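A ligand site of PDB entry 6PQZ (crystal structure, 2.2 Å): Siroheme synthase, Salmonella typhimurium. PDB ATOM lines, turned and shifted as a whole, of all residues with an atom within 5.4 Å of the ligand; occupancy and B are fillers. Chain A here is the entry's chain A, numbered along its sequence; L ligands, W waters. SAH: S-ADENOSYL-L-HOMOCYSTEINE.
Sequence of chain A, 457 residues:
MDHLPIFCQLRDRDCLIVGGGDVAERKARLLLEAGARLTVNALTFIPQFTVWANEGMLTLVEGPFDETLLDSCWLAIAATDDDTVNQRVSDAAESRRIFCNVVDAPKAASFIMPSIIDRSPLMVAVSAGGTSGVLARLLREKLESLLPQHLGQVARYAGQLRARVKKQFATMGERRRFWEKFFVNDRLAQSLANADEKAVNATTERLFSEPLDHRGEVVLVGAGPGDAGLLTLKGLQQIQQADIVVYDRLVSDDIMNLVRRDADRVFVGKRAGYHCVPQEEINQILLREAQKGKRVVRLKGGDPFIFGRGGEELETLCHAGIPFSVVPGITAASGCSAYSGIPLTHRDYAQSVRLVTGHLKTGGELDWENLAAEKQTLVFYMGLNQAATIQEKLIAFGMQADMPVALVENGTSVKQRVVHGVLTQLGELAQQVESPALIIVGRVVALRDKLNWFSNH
Water W1 lies within hydrogen-bond range of a nitrogen (N7) of the ligand (2.7 Å) and the backbone carbonyl oxygen of Leu 250 (2.9 Å).
Water W2 lies within hydrogen-bond range of OG of Ser 435 (2.9 Å), N of Ala 437 (3.0 Å) and O3' of the ligand (3.2 Å).
The backbone NH (N) of Ala 333 lies within hydrogen-bond range of the side-chain hydroxyl (OH) of Tyr 381 (3.0 Å).
The side-chain hydroxyl of Thr 331 lies within hydrogen-bond range of the side-chain hydroxyl of Tyr 381 (2.9 Å).
The backbone carbonyl oxygen (O) of Pro 436 is in hydrogen-bond range of the backbone NH (N) of Asn 410 (3.0 Å).
The backbone carbonyl oxygen (O) of Ala 332 lies close to the side-chain sulfur (SG) of Cys 336 (3.2 Å).
O of Val 408 sits at hydrogen-bond distance from N of Leu 438, 2.9 Å away.
SD of the ligand lies close to O of Phe 307 (3.5 Å).
Leu 250 touches the ligand.
CA of Gly 302 touches C of the ligand, 3.5 Å away.
Tyr 381 touches the ligand (CE2 to OXT, 3.3 Å).
O of Val 408 touches C2 of the ligand (3.1 Å).
Asn 410 touches the ligand.
O of Pro 436 touches C2 of the ligand, 3.6 Å away.
Hydrophobic or aromatic side chains that line the ligand: Pro 225, Leu 250, Ile 306, Ala 332, Tyr 381, Met 382 and Leu 438.
Within 4 Å of the ligand: Pro 225, Leu 250, Gly 301, Gly 302, Asp 303, Ile 306, Phe 307, Thr 331, Ala 332, Cys 336, Tyr 381, Met 382, Val 408, Asn 410, Gly 411, Pro 436, Ala 437 and Leu 438.
The nearest printed residue that does not touch the ligand is Gly 308 (4.2 Å).
O of the ligand sits at hydrogen-bond distance from OG1 of Thr 331.
N6 of the ligand is in hydrogen-bond range of O of Pro 225, 2.8 Å away.
N of Ala 332 lies within hydrogen-bond range of OXT of the ligand.
The backbone NH of Met 382 lies within hydrogen-bond range of an oxygen (O2') of the ligand (3.0 Å).
The backbone carbonyl oxygen (O) of Ala 437 sits at hydrogen-bond distance from an oxygen (O2') of the ligand, 2.6 Å away.
N of the ligand lies close to O of Gly 301, at 3.3 Å.
SG of Cys 336 sits close to N1 of the ligand.
A nitrogen (N) of the ligand is in hydrogen-bond range of the backbone carbonyl oxygen of Asp 303, 2.8 Å away.
The backbone NH (N) of Leu 438 is in hydrogen-bond range of a nitrogen (N3) of the ligand (3.4 Å).
The backbone carbonyl oxygen (O) of Gly 411 is in hydrogen-bond range of a nitrogen (N6) of the ligand.
O of Ile 306 sits at hydrogen-bond distance from N of the ligand, at 2.7 Å.
The backbone NH of Gly 411 lies within hydrogen-bond range of a nitrogen (N1) of the ligand.
An oxygen (O) of the ligand lies within hydrogen-bond range of the backbone NH of Asp 303 (2.8 Å).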
ATOM      1  N   PRO A 225     -27.915   9.374 -16.729  1.00  0.00           N
ATOM      2  CA  PRO A 225     -26.453   9.395 -16.748  1.00  0.00           C
ATOM      3  C   PRO A 225     -25.794   8.757 -15.538  1.00  0.00           C
ATOM      4  O   PRO A 225     -24.565   8.583 -15.544  1.00  0.00           O
ATOM      5  CB  PRO A 225     -26.135  10.889 -16.825  1.00  0.00           C
ATOM      6  CG  PRO A 225     -27.296  11.554 -16.222  1.00  0.00           C
ATOM      7  CD  PRO A 225     -28.492  10.666 -16.314  1.00  0.00           C
ATOM      8  N   GLY A 226     -26.535   8.364 -14.523  1.00  0.00           N
ATOM      9  CA  GLY A 226     -25.889   7.684 -13.421  1.00  0.00           C
ATOM     10  C   GLY A 226     -26.683   7.714 -12.136  1.00  0.00           C
ATOM     11  O   GLY A 226     -26.942   6.667 -11.550  1.00  0.00           O
ATOM     12  N   LEU A 250     -22.006   1.963 -19.091  1.00  0.00           N
ATOM     13  CA  LEU A 250     -22.538   3.308 -18.905  1.00  0.00           C
ATOM     14  C   LEU A 250     -23.856   3.328 -18.174  1.00  0.00           C
ATOM     15  O   LEU A 250     -24.414   4.409 -17.944  1.00  0.00           O
ATOM     16  CB  LEU A 250     -22.693   4.011 -20.262  1.00  0.00           C
ATOM     17  CG  LEU A 250     -21.366   4.540 -20.784  1.00  0.00           C
ATOM     18  CD1 LEU A 250     -21.573   5.499 -21.929  1.00  0.00           C
ATOM     19  CD2 LEU A 250     -20.618   5.222 -19.656  1.00  0.00           C
ATOM     20  N   GLY A 301     -27.088   3.912 -21.134  1.00  0.00           N
ATOM     21  CA  GLY A 301     -26.775   5.155 -20.465  1.00  0.00           C
ATOM     22  C   GLY A 301     -27.488   6.301 -21.147  1.00  0.00           C
ATOM     23  O   GLY A 301     -27.708   6.294 -22.358  1.00  0.00           O
ATOM     24  N   GLY A 302     -27.923   7.278 -20.339  1.00  0.00           N
ATOM     25  CA  GLY A 302     -28.414   8.508 -20.936  1.00  0.00           C
ATOM     26  C   GLY A 302     -29.764   8.273 -21.571  1.00  0.00           C
ATOM     27  O   GLY A 302     -30.639   7.637 -20.997  1.00  0.00           O
ATOM     28  N   ASP A 303     -29.935   8.802 -22.828  1.00  0.00           N
ATOM     29  CA  ASP A 303     -31.059   8.669 -23.747  1.00  0.00           C
ATOM     30  C   ASP A 303     -30.698   7.718 -24.872  1.00  0.00           C
ATOM     31  O   ASP A 303     -29.633   7.890 -25.493  1.00  0.00           O
ATOM     32  CB  ASP A 303     -31.460  10.022 -24.324  1.00  0.00           C
ATOM     33  CG  ASP A 303     -32.734   9.947 -25.176  1.00  0.00           C
ATOM     34  OD1 ASP A 303     -32.642   9.958 -26.423  1.00  0.00           O
ATOM     35  OD2 ASP A 303     -33.830   9.864 -24.587  1.00  0.00           O
ATOM     36  N   PRO A 304     -31.566   6.746 -25.175  1.00  0.00           N
ATOM     37  CA  PRO A 304     -31.237   5.719 -26.174  1.00  0.00           C
ATOM     38  C   PRO A 304     -30.992   6.258 -27.559  1.00  0.00           C
ATOM     39  O   PRO A 304     -30.274   5.624 -28.336  1.00  0.00           O
ATOM     40  CB  PRO A 304     -32.461   4.801 -26.161  1.00  0.00           C
ATOM     41  CG  PRO A 304     -33.143   5.068 -24.860  1.00  0.00           C
ATOM     42  CD  PRO A 304     -32.885   6.514 -24.559  1.00  0.00           C
ATOM     43  N   ILE A 306     -29.645   9.299 -28.463  1.00  0.00           N
ATOM     44  CA  ILE A 306     -28.613  10.315 -28.604  1.00  0.00           C
ATOM     45  C   ILE A 306     -27.273   9.588 -28.546  1.00  0.00           C
ATOM     46  O   ILE A 306     -26.784   9.227 -27.465  1.00  0.00           O
ATOM     47  CB  ILE A 306     -28.731  11.408 -27.532  1.00  0.00           C
ATOM     48  CG1 ILE A 306     -29.961  12.262 -27.842  1.00  0.00           C
ATOM     49  CG2 ILE A 306     -27.498  12.304 -27.547  1.00  0.00           C
ATOM     50  CD1 ILE A 306     -30.610  12.902 -26.631  1.00  0.00           C
ATOM     51  N   PHE A 307     -26.672   9.366 -29.716  1.00  0.00           N
ATOM     52  CA  PHE A 307     -25.414   8.624 -29.825  1.00  0.00           C
ATOM     53  C   PHE A 307     -25.521   7.272 -29.135  1.00  0.00           C
ATOM     54  O   PHE A 307     -24.580   6.800 -28.490  1.00  0.00           O
ATOM     55  CB  PHE A 307     -24.246   9.445 -29.271  1.00  0.00           C
ATOM     56  CG  PHE A 307     -24.149  10.817 -29.872  1.00  0.00           C
ATOM     57  CD1 PHE A 307     -23.819  10.955 -31.212  1.00  0.00           C
ATOM     58  CD2 PHE A 307     -24.399  11.946 -29.116  1.00  0.00           C
ATOM     59  CE1 PHE A 307     -23.733  12.220 -31.789  1.00  0.00           C
ATOM     60  CE2 PHE A 307     -24.308  13.207 -29.684  1.00  0.00           C
ATOM     61  CZ  PHE A 307     -23.979  13.348 -31.010  1.00  0.00           C
ATOM     62  N   GLY A 308     -26.676   6.636 -29.260  1.00  0.00           N
ATOM     63  CA  GLY A 308     -26.921   5.423 -28.515  1.00  0.00           C
ATOM     64  C   GLY A 308     -26.811   4.155 -29.342  1.00  0.00           C
ATOM     65  O   GLY A 308     -26.847   3.058 -28.777  1.00  0.00           O
ATOM     66  N   ILE A 330     -32.767  10.854 -19.369  1.00  0.00           N
ATOM     67  CA  ILE A 330     -32.018  12.085 -19.197  1.00  0.00           C
ATOM     68  C   ILE A 330     -30.695  11.864 -19.915  1.00  0.00           C
ATOM     69  O   ILE A 330     -29.903  11.001 -19.514  1.00  0.00           O
ATOM     70  CB  ILE A 330     -31.808  12.413 -17.710  1.00  0.00           C
ATOM     71  CG1 ILE A 330     -33.139  12.446 -16.953  1.00  0.00           C
ATOM     72  CG2 ILE A 330     -31.023  13.717 -17.555  1.00  0.00           C
ATOM     73  CD1 ILE A 330     -34.044  13.507 -17.401  1.00  0.00           C
ATOM     74  N   THR A 331     -30.460  12.594 -21.002  1.00  0.00           N
ATOM     75  CA  THR A 331     -29.205  12.407 -21.702  1.00  0.00           C
ATOM     76  C   THR A 331     -28.047  13.004 -20.873  1.00  0.00           C
ATOM     77  O   THR A 331     -28.248  13.803 -19.972  1.00  0.00           O
ATOM     78  CB  THR A 331     -29.283  13.039 -23.085  1.00  0.00           C
ATOM     79  OG1 THR A 331     -28.198  12.550 -23.880  1.00  0.00           O
ATOM     80  CG2 THR A 331     -29.221  14.552 -22.972  1.00  0.00           C
ATOM     81  N   ALA A 332     -26.821  12.559 -21.164  1.00  0.00           N
ATOM     82  CA  ALA A 332     -25.689  13.030 -20.359  1.00  0.00           C
ATOM     83  C   ALA A 332     -25.637  14.557 -20.321  1.00  0.00           C
ATOM     84  O   ALA A 332     -25.350  15.150 -19.269  1.00  0.00           O
ATOM     85  CB  ALA A 332     -24.378  12.467 -20.912  1.00  0.00           C
ATOM     86  N   ALA A 333     -25.976  15.222 -21.430  1.00  0.00           N
ATOM     87  CA  ALA A 333     -25.949  16.682 -21.454  1.00  0.00           C
ATOM     88  C   ALA A 333     -26.880  17.294 -20.405  1.00  0.00           C
ATOM     89  O   ALA A 333     -26.470  18.183 -19.656  1.00  0.00           O
ATOM     90  CB  ALA A 333     -26.309  17.199 -22.849  1.00  0.00           C
ATOM     91  N   CYS A 336     -25.550  16.245 -16.766  1.00  0.00           N
ATOM     92  CA  CYS A 336     -24.348  16.997 -16.435  1.00  0.00           C
ATOM     93  C   CYS A 336     -24.667  18.465 -16.243  1.00  0.00           C
ATOM     94  O   CYS A 336     -24.190  19.082 -15.286  1.00  0.00           O
ATOM     95  CB  CYS A 336     -23.293  16.792 -17.517  1.00  0.00           C
ATOM     96  SG  CYS A 336     -22.660  15.121 -17.476  1.00  0.00           S
ATOM     97  N   PHE A 380     -19.832  17.753 -26.329  1.00  0.00           N
ATOM     98  CA  PHE A 380     -19.153  16.673 -27.018  1.00  0.00           C
ATOM     99  C   PHE A 380     -19.286  15.397 -26.206  1.00  0.00           C
ATOM    100  O   PHE A 380     -18.941  15.360 -25.015  1.00  0.00           O
ATOM    101  CB  PHE A 380     -17.676  16.988 -27.236  1.00  0.00           C
ATOM    102  CG  PHE A 380     -17.467  18.089 -28.180  1.00  0.00           C
ATOM    103  CD1 PHE A 380     -17.521  19.396 -27.744  1.00  0.00           C
ATOM    104  CD2 PHE A 380     -17.236  17.809 -29.520  1.00  0.00           C
ATOM    105  CE1 PHE A 380     -17.322  20.418 -28.639  1.00  0.00           C
ATOM    106  CE2 PHE A 380     -17.050  18.830 -30.408  1.00  0.00           C
ATOM    107  CZ  PHE A 380     -17.104  20.137 -29.972  1.00  0.00           C
ATOM    108  N   TYR A 381     -19.791  14.376 -26.852  1.00  0.00           N
ATOM    109  CA  TYR A 381     -19.926  13.060 -26.292  1.00  0.00           C
ATOM    110  C   TYR A 381     -18.754  12.214 -26.776  1.00  0.00           C
ATOM    111  O   TYR A 381     -18.414  12.257 -27.963  1.00  0.00           O
ATOM    112  CB  TYR A 381     -21.236  12.425 -26.756  1.00  0.00           C
ATOM    113  CG  TYR A 381     -22.471  12.962 -26.086  1.00  0.00           C
ATOM    114  CD1 TYR A 381     -22.841  14.288 -26.232  1.00  0.00           C
ATOM    115  CD2 TYR A 381     -23.276  12.128 -25.338  1.00  0.00           C
ATOM    116  CE1 TYR A 381     -23.988  14.766 -25.641  1.00  0.00           C
ATOM    117  CE2 TYR A 381     -24.413  12.600 -24.730  1.00  0.00           C
ATOM    118  CZ  TYR A 381     -24.777  13.918 -24.896  1.00  0.00           C
ATOM    119  OH  TYR A 381     -25.916  14.365 -24.284  1.00  0.00           O
ATOM    120  N   MET A 382     -18.197  11.416 -25.868  1.00  0.00           N
ATOM    121  CA  MET A 382     -17.018  10.576 -26.131  1.00  0.00           C
ATOM    122  C   MET A 382     -15.981  11.334 -26.953  1.00  0.00           C
ATOM    123  O   MET A 382     -15.493  10.869 -27.981  1.00  0.00           O
ATOM    124  CB  MET A 382     -17.409   9.243 -26.789  1.00  0.00           C
ATOM    125  CG  MET A 382     -18.251   9.316 -28.058  1.00  0.00           C
ATOM    126  SD  MET A 382     -19.131   7.805 -28.514  1.00  0.00           S
ATOM    127  CE  MET A 382     -20.418   8.533 -29.525  1.00  0.00           C
ATOM    128  N   GLY A 383     -15.674  12.543 -26.494  1.00  0.00           N
ATOM    129  CA  GLY A 383     -14.668  13.361 -27.149  1.00  0.00           C
ATOM    130  C   GLY A 383     -13.335  13.463 -26.420  1.00  0.00           C
ATOM    131  O   GLY A 383     -12.466  14.211 -26.870  1.00  0.00           O
ATOM    132  N   VAL A 408     -17.178  17.168 -17.439  1.00  0.00           N
ATOM    133  CA  VAL A 408     -17.952  16.569 -16.376  1.00  0.00           C
ATOM    134  C   VAL A 408     -17.722  15.085 -16.470  1.00  0.00           C
ATOM    135  O   VAL A 408     -18.086  14.457 -17.477  1.00  0.00           O
ATOM    136  CB  VAL A 408     -19.433  16.948 -16.491  1.00  0.00           C
ATOM    137  CG1 VAL A 408     -20.226  16.322 -15.354  1.00  0.00           C
ATOM    138  CG2 VAL A 408     -19.549  18.470 -16.476  1.00  0.00           C
ATOM    139  N   GLU A 409     -17.040  14.534 -15.475  1.00  0.00           N
ATOM    140  CA  GLU A 409     -16.796  13.113 -15.377  1.00  0.00           C
ATOM    141  C   GLU A 409     -17.833  12.516 -14.439  1.00  0.00           C
ATOM    142  O   GLU A 409     -17.991  12.999 -13.308  1.00  0.00           O
ATOM    143  CB  GLU A 409     -15.408  12.827 -14.831  1.00  0.00           C
ATOM    144  CG  GLU A 409     -15.058  11.362 -14.892  1.00  0.00           C
ATOM    145  CD  GLU A 409     -13.709  11.062 -14.302  1.00  0.00           C
ATOM    146  OE1 GLU A 409     -13.112  11.972 -13.696  1.00  0.00           O
ATOM    147  OE2 GLU A 409     -13.233   9.918 -14.432  1.00  0.00           O
ATOM    148  N   ASN A 410     -18.496  11.443 -14.884  1.00  0.00           N
ATOM    149  CA  ASN A 410     -19.459  10.743 -14.046  1.00  0.00           C
ATOM    150  C   ASN A 410     -20.495  11.729 -13.512  1.00  0.00           C
ATOM    151  O   ASN A 410     -20.776  11.784 -12.309  1.00  0.00           O
ATOM    152  CB  ASN A 410     -18.750  10.012 -12.918  1.00  0.00           C
ATOM    153  CG  ASN A 410     -17.918   8.862 -13.406  1.00  0.00           C
ATOM    154  OD1 ASN A 410     -18.424   7.982 -14.106  1.00  0.00           O
ATOM    155  ND2 ASN A 410     -16.634   8.867 -13.073  1.00  0.00           N
ATOM    156  N   GLY A 411     -21.010  12.559 -14.409  1.00  0.00           N
ATOM    157  CA  GLY A 411     -22.000  13.540 -14.030  1.00  0.00           C
ATOM    158  C   GLY A 411     -23.165  12.848 -13.363  1.00  0.00           C
ATOM    159  O   GLY A 411     -23.548  11.751 -13.766  1.00  0.00           O
ATOM    160  N   THR A 412     -23.709  13.482 -12.331  1.00  0.00           N
ATOM    161  CA  THR A 412     -24.859  13.072 -11.531  1.00  0.00           C
ATOM    162  C   THR A 412     -24.557  11.946 -10.540  1.00  0.00           C
ATOM    163  O   THR A 412     -25.470  11.566  -9.774  1.00  0.00           O
ATOM    164  CB  THR A 412     -26.057  12.613 -12.378  1.00  0.00           C
ATOM    165  OG1 THR A 412     -25.824  11.270 -12.827  1.00  0.00           O
ATOM    166  CG2 THR A 412     -26.277  13.564 -13.580  1.00  0.00           C
ATOM    167  N   SER A 435     -12.982   8.639 -18.885  1.00  0.00           N
ATOM    168  CA  SER A 435     -14.305   8.219 -19.315  1.00  0.00           C
ATOM    169  C   SER A 435     -15.078   7.676 -18.118  1.00  0.00           C
ATOM    170  O   SER A 435     -14.512   6.996 -17.266  1.00  0.00           O
ATOM    171  CB  SER A 435     -14.205   7.165 -20.409  1.00  0.00           C
ATOM    172  OG  SER A 435     -13.765   7.758 -21.604  1.00  0.00           O
ATOM    173  N   PRO A 436     -16.390   7.973 -18.023  1.00  0.00           N
ATOM    174  CA  PRO A 436     -17.139   8.768 -19.013  1.00  0.00           C
ATOM    175  C   PRO A 436     -17.170  10.240 -18.697  1.00  0.00           C
ATOM    176  O   PRO A 436     -17.517  10.621 -17.568  1.00  0.00           O
ATOM    177  CB  PRO A 436     -18.548   8.177 -18.938  1.00  0.00           C
ATOM    178  CG  PRO A 436     -18.602   7.370 -17.633  1.00  0.00           C
ATOM    179  CD  PRO A 436     -17.267   7.450 -16.965  1.00  0.00           C
ATOM    180  N   ALA A 437     -16.864  11.064 -19.703  1.00  0.00           N
ATOM    181  CA  ALA A 437     -16.801  12.505 -19.520  1.00  0.00           C
ATOM    182  C   ALA A 437     -17.469  13.223 -20.680  1.00  0.00           C
ATOM    183  O   ALA A 437     -17.362  12.806 -21.838  1.00  0.00           O
ATOM    184  CB  ALA A 437     -15.355  13.006 -19.406  1.00  0.00           C
ATOM    185  N   LEU A 438     -18.131  14.326 -20.352  1.00  0.00           N
ATOM    186  CA  LEU A 438     -18.727  15.231 -21.317  1.00  0.00           C
ATOM    187  C   LEU A 438     -17.860  16.476 -21.399  1.00  0.00           C
ATOM    188  O   LEU A 438     -17.331  16.935 -20.389  1.00  0.00           O
ATOM    189  CB  LEU A 438     -20.120  15.640 -20.864  1.00  0.00           C
ATOM    190  CG  LEU A 438     -21.296  15.630 -21.801  1.00  0.00           C
ATOM    191  CD1 LEU A 438     -21.535  14.238 -22.290  1.00  0.00           C
ATOM    192  CD2 LEU A 438     -22.495  16.157 -21.069  1.00  0.00           C
HETATM  193  N   SAH L   1     -26.858   7.861 -25.096  1.00  0.00           N
HETATM  194  CA  SAH L   1     -26.073   8.504 -24.031  1.00  0.00           C
HETATM  195  CB  SAH L   1     -24.636   8.724 -24.452  1.00  0.00           C
HETATM  196  CG  SAH L   1     -24.020   7.565 -25.246  1.00  0.00           C
HETATM  197  SD  SAH L   1     -22.397   7.987 -25.970  1.00  0.00           S
HETATM  198  C   SAH L   1     -26.687   9.842 -23.612  1.00  0.00           C
HETATM  199  O   SAH L   1     -27.782  10.163 -24.075  1.00  0.00           O
HETATM  200  OXT SAH L   1     -26.117  10.599 -22.816  1.00  0.00           O
HETATM  201  C5' SAH L   1     -21.453   7.844 -24.432  1.00  0.00           C
HETATM  202  C4' SAH L   1     -20.864   9.176 -24.020  1.00  0.00           C
HETATM  203  O4' SAH L   1     -21.819   9.868 -23.260  1.00  0.00           O
HETATM  204  C3' SAH L   1     -19.623   9.084 -23.142  1.00  0.00           C
HETATM  205  O3' SAH L   1     -18.438   9.044 -23.899  1.00  0.00           O
HETATM  206  C2' SAH L   1     -19.683  10.360 -22.342  1.00  0.00           C
HETATM  207  O2' SAH L   1     -19.160  11.455 -23.058  1.00  0.00           O
HETATM  208  C1' SAH L   1     -21.178  10.615 -22.250  1.00  0.00           C
HETATM  209  N9  SAH L   1     -21.684  10.255 -20.918  1.00  0.00           N
HETATM  210  C8  SAH L   1     -22.524   9.218 -20.568  1.00  0.00           C
HETATM  211  N7  SAH L   1     -22.725   9.300 -19.229  1.00  0.00           N
HETATM  212  C5  SAH L   1     -22.020  10.354 -18.742  1.00  0.00           C
HETATM  213  C6  SAH L   1     -21.860  10.872 -17.470  1.00  0.00           C
HETATM  214  N6  SAH L   1     -22.482  10.312 -16.434  1.00  0.00           N
HETATM  215  N1  SAH L   1     -21.058  11.978 -17.294  1.00  0.00           N
HETATM  216  C2  SAH L   1     -20.425  12.580 -18.344  1.00  0.00           C
HETATM  217  N3  SAH L   1     -20.587  12.051 -19.607  1.00  0.00           N
HETATM  218  C4  SAH L   1     -21.363  10.962 -19.791  1.00  0.00           C
HETATM  219  O   HOH W   1     -24.406   7.168 -18.901  1.00  0.00           O
HETATM  220  O   HOH W   2     -15.874   9.660 -22.173  1.00  0.00           O
